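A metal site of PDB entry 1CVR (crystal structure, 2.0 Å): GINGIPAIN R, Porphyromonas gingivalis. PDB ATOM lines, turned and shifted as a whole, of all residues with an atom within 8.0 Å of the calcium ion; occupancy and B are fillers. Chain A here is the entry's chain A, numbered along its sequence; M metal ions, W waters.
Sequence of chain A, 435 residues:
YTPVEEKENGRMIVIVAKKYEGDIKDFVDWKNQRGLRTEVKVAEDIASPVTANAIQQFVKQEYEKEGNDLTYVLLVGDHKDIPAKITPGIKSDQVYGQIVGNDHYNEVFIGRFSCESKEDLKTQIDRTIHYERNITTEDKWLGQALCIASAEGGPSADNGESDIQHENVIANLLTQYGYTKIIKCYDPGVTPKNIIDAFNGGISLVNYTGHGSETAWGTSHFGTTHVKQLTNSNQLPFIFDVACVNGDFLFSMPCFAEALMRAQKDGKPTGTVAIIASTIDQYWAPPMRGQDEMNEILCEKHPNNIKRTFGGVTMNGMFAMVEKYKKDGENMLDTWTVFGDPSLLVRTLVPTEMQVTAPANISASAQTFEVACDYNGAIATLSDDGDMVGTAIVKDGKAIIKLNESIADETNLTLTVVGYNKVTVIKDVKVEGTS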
ATOM      1  N   TYR A  63     -14.415 -14.689 -22.512  1.00  0.00           N
ATOM      2  CA  TYR A  63     -13.181 -14.075 -23.001  1.00  0.00           C
ATOM      3  C   TYR A  63     -12.043 -14.282 -22.008  1.00  0.00           C
ATOM      4  O   TYR A  63     -10.894 -14.484 -22.400  1.00  0.00           O
ATOM      5  CB  TYR A  63     -13.373 -12.567 -23.214  1.00  0.00           C
ATOM      6  CG  TYR A  63     -12.124 -11.854 -23.704  1.00  0.00           C
ATOM      7  CD1 TYR A  63     -11.711 -11.956 -25.042  1.00  0.00           C
ATOM      8  CD2 TYR A  63     -11.336 -11.117 -22.834  1.00  0.00           C
ATOM      9  CE1 TYR A  63     -10.541 -11.339 -25.481  1.00  0.00           C
ATOM     10  CE2 TYR A  63     -10.165 -10.490 -23.273  1.00  0.00           C
ATOM     11  CZ  TYR A  63      -9.779 -10.611 -24.595  1.00  0.00           C
ATOM     12  OH  TYR A  63      -8.630  -9.983 -25.031  1.00  0.00           O
ATOM     13  N   GLY A  97     -18.376  -6.580 -27.105  1.00  0.00           N
ATOM     14  CA  GLY A  97     -17.003  -6.991 -27.349  1.00  0.00           C
ATOM     15  C   GLY A  97     -15.949  -6.052 -26.768  1.00  0.00           C
ATOM     16  O   GLY A  97     -14.758  -6.210 -27.059  1.00  0.00           O
ATOM     17  N   GLN A  98     -16.381  -5.070 -25.982  1.00  0.00           N
ATOM     18  CA  GLN A  98     -15.464  -4.105 -25.340  1.00  0.00           C
ATOM     19  C   GLN A  98     -15.309  -4.613 -23.915  1.00  0.00           C
ATOM     20  O   GLN A  98     -16.142  -4.360 -23.037  1.00  0.00           O
ATOM     21  CB  GLN A  98     -16.083  -2.711 -25.378  1.00  0.00           C
ATOM     22  CG  GLN A  98     -15.972  -2.046 -26.748  1.00  0.00           C
ATOM     23  CD  GLN A  98     -16.998  -0.949 -26.926  1.00  0.00           C
ATOM     24  OE1 GLN A  98     -17.355  -0.263 -25.979  1.00  0.00           O
ATOM     25  NE2 GLN A  98     -17.480  -0.776 -28.150  1.00  0.00           N
ATOM     26  N   ILE A  99     -14.187  -5.290 -23.690  1.00  0.00           N
ATOM     27  CA  ILE A  99     -13.931  -5.957 -22.431  1.00  0.00           C
ATOM     28  C   ILE A  99     -12.748  -5.471 -21.589  1.00  0.00           C
ATOM     29  O   ILE A  99     -12.835  -5.411 -20.369  1.00  0.00           O
ATOM     30  CB  ILE A  99     -13.734  -7.466 -22.739  1.00  0.00           C
ATOM     31  CG1 ILE A  99     -14.881  -7.935 -23.639  1.00  0.00           C
ATOM     32  CG2 ILE A  99     -13.681  -8.297 -21.455  1.00  0.00           C
ATOM     33  CD1 ILE A  99     -14.703  -9.342 -24.175  1.00  0.00           C
ATOM     34  N   VAL A 100     -11.656  -5.122 -22.266  1.00  0.00           N
ATOM     35  CA  VAL A 100     -10.428  -4.703 -21.592  1.00  0.00           C
ATOM     36  C   VAL A 100      -9.901  -3.328 -21.967  1.00  0.00           C
ATOM     37  O   VAL A 100     -10.041  -2.899 -23.116  1.00  0.00           O
ATOM     38  CB  VAL A 100      -9.288  -5.711 -21.900  1.00  0.00           C
ATOM     39  CG1 VAL A 100      -7.965  -5.209 -21.347  1.00  0.00           C
ATOM     40  CG2 VAL A 100      -9.634  -7.063 -21.332  1.00  0.00           C
ATOM     41  N   GLY A 101      -9.259  -2.664 -21.005  1.00  0.00           N
ATOM     42  CA  GLY A 101      -8.652  -1.376 -21.262  1.00  0.00           C
ATOM     43  C   GLY A 101      -9.465  -0.118 -21.034  1.00  0.00           C
ATOM     44  O   GLY A 101      -8.998   0.960 -21.352  1.00  0.00           O
ATOM     45  N   ASN A 102     -10.665  -0.249 -20.472  1.00  0.00           N
ATOM     46  CA  ASN A 102     -11.514   0.901 -20.219  1.00  0.00           C
ATOM     47  C   ASN A 102     -11.556   1.826 -21.418  1.00  0.00           C
ATOM     48  O   ASN A 102     -11.273   3.025 -21.318  1.00  0.00           O
ATOM     49  CB  ASN A 102     -11.011   1.689 -18.996  1.00  0.00           C
ATOM     50  CG  ASN A 102     -11.202   0.943 -17.692  1.00  0.00           C
ATOM     51  OD1 ASN A 102     -10.277   0.363 -17.146  1.00  0.00           O
ATOM     52  ND2 ASN A 102     -12.442   0.930 -17.202  1.00  0.00           N
ATOM     53  N   ASP A 103     -11.912   1.269 -22.573  1.00  0.00           N
ATOM     54  CA  ASP A 103     -11.974   2.033 -23.791  1.00  0.00           C
ATOM     55  C   ASP A 103     -13.011   1.429 -24.732  1.00  0.00           C
ATOM     56  O   ASP A 103     -13.670   0.466 -24.392  1.00  0.00           O
ATOM     57  CB  ASP A 103     -10.586   2.076 -24.444  1.00  0.00           C
ATOM     58  CG  ASP A 103     -10.072   0.699 -24.801  1.00  0.00           C
ATOM     59  OD1 ASP A 103      -8.836   0.519 -24.848  1.00  0.00           O
ATOM     60  OD2 ASP A 103     -10.883  -0.213 -25.051  1.00  0.00           O
ATOM     61  N   HIS A 104     -13.151   2.007 -25.909  1.00  0.00           N
ATOM     62  CA  HIS A 104     -14.133   1.511 -26.864  1.00  0.00           C
ATOM     63  C   HIS A 104     -13.513   0.693 -27.984  1.00  0.00           C
ATOM     64  O   HIS A 104     -14.157   0.457 -29.002  1.00  0.00           O
ATOM     65  CB  HIS A 104     -14.926   2.689 -27.413  1.00  0.00           C
ATOM     66  CG  HIS A 104     -15.746   3.379 -26.377  1.00  0.00           C
ATOM     67  ND1 HIS A 104     -17.081   3.087 -26.151  1.00  0.00           N
ATOM     68  CD2 HIS A 104     -15.389   4.250 -25.395  1.00  0.00           C
ATOM     69  CE1 HIS A 104     -17.505   3.759 -25.102  1.00  0.00           C
ATOM     70  NE2 HIS A 104     -16.497   4.466 -24.616  1.00  0.00           N
ATOM     71  N   TYR A 105     -12.259   0.281 -27.812  1.00  0.00           N
ATOM     72  CA  TYR A 105     -11.601  -0.544 -28.814  1.00  0.00           C
ATOM     73  C   TYR A 105     -11.974  -1.985 -28.510  1.00  0.00           C
ATOM     74  O   TYR A 105     -11.515  -2.548 -27.521  1.00  0.00           O
ATOM     75  CB  TYR A 105     -10.072  -0.376 -28.757  1.00  0.00           C
ATOM     76  CG  TYR A 105      -9.564   0.977 -29.179  1.00  0.00           C
ATOM     77  CD1 TYR A 105      -9.726   1.440 -30.480  1.00  0.00           C
ATOM     78  CD2 TYR A 105      -8.917   1.819 -28.259  1.00  0.00           C
ATOM     79  CE1 TYR A 105      -9.263   2.696 -30.871  1.00  0.00           C
ATOM     80  CE2 TYR A 105      -8.448   3.085 -28.643  1.00  0.00           C
ATOM     81  CZ  TYR A 105      -8.625   3.518 -29.945  1.00  0.00           C
ATOM     82  OH  TYR A 105      -8.212   4.776 -30.305  1.00  0.00           O
ATOM     83  N   ASN A 106     -12.813  -2.589 -29.340  1.00  0.00           N
ATOM     84  CA  ASN A 106     -13.216  -3.973 -29.125  1.00  0.00           C
ATOM     85  C   ASN A 106     -12.077  -4.987 -29.055  1.00  0.00           C
ATOM     86  O   ASN A 106     -11.040  -4.816 -29.693  1.00  0.00           O
ATOM     87  CB  ASN A 106     -14.162  -4.456 -30.232  1.00  0.00           C
ATOM     88  CG  ASN A 106     -15.572  -3.947 -30.073  1.00  0.00           C
ATOM     89  OD1 ASN A 106     -15.800  -2.743 -29.867  1.00  0.00           O
ATOM     90  ND2 ASN A 106     -16.549  -4.850 -30.173  1.00  0.00           N
ATOM     91  N   GLU A 107     -12.304  -6.022 -28.262  1.00  0.00           N
ATOM     92  CA  GLU A 107     -11.389  -7.148 -28.109  1.00  0.00           C
ATOM     93  C   GLU A 107     -11.995  -8.268 -28.941  1.00  0.00           C
ATOM     94  O   GLU A 107     -11.266  -9.116 -29.468  1.00  0.00           O
ATOM     95  CB  GLU A 107     -11.340  -7.653 -26.666  1.00  0.00           C
ATOM     96  CG  GLU A 107     -10.308  -6.992 -25.794  1.00  0.00           C
ATOM     97  CD  GLU A 107     -10.550  -5.519 -25.632  1.00  0.00           C
ATOM     98  OE1 GLU A 107     -11.572  -5.142 -25.029  1.00  0.00           O
ATOM     99  OE2 GLU A 107      -9.708  -4.746 -26.117  1.00  0.00           O
ATOM    100  N   VAL A 108     -13.319  -8.224 -29.084  1.00  0.00           N
ATOM    101  CA  VAL A 108     -14.094  -9.274 -29.777  1.00  0.00           C
ATOM    102  C   VAL A 108     -15.007  -8.706 -30.871  1.00  0.00           C
ATOM    103  O   VAL A 108     -15.658  -7.672 -30.669  1.00  0.00           O
ATOM    104  CB  VAL A 108     -14.955 -10.064 -28.714  1.00  0.00           C
ATOM    105  CG1 VAL A 108     -15.836 -11.122 -29.387  1.00  0.00           C
ATOM    106  CG2 VAL A 108     -14.022 -10.725 -27.675  1.00  0.00           C
ATOM    107  N   PHE A 319     -11.498   1.895 -35.751  1.00  0.00           N
ATOM    108  CA  PHE A 319     -10.477   2.310 -34.784  1.00  0.00           C
ATOM    109  C   PHE A 319      -9.846   3.629 -35.233  1.00  0.00           C
ATOM    110  O   PHE A 319      -9.545   4.495 -34.417  1.00  0.00           O
ATOM    111  CB  PHE A 319      -9.374   1.249 -34.655  1.00  0.00           C
ATOM    112  CG  PHE A 319      -9.726   0.090 -33.770  1.00  0.00           C
ATOM    113  CD1 PHE A 319     -11.040  -0.124 -33.346  1.00  0.00           C
ATOM    114  CD2 PHE A 319      -8.732  -0.807 -33.353  1.00  0.00           C
ATOM    115  CE1 PHE A 319     -11.356  -1.215 -32.521  1.00  0.00           C
ATOM    116  CE2 PHE A 319      -9.039  -1.899 -32.533  1.00  0.00           C
ATOM    117  CZ  PHE A 319     -10.358  -2.103 -32.119  1.00  0.00           C
HETATM  118 CA    CA M   1     -10.661  -2.591 -25.330  1.00  0.00          CA
HETATM  119  O   HOH W   1      -8.443  -2.007 -25.749  1.00  0.00           O
HETATM  120  O   HOH W   2     -12.752  -2.209 -24.438  1.00  0.00           O
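N of Ile 99 lies close to OE1 of Glu 107 (2.9 Å).
N of Glu 107 sits at hydrogen-bond distance from O of Gly 97, 2.7 Å away.
Of the 14 residues printed, 4 come within 4 Å of the calcium ion.
The nearest printed residue that does not touch the calcium ion is Gly 101 (4.5 Å).
The calcium ion is bound by water W2 (2.3 Å), the backbone carbonyl oxygen (O) of Val 100 (2.3 Å), water W1 (2.3 Å), the backbone carbonyl oxygen (O) of Tyr 105 (2.4 Å), the side-chain carboxylate (OD2) of Asp 103 (2.4 Å), the side-chain carboxylate (OE2) of Glu 107 (2.5 Å) and the side-chain carboxylate (OE1) of Glu 107 (2.7 Å).
The calcium ion has seven donor atoms within binding distance.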
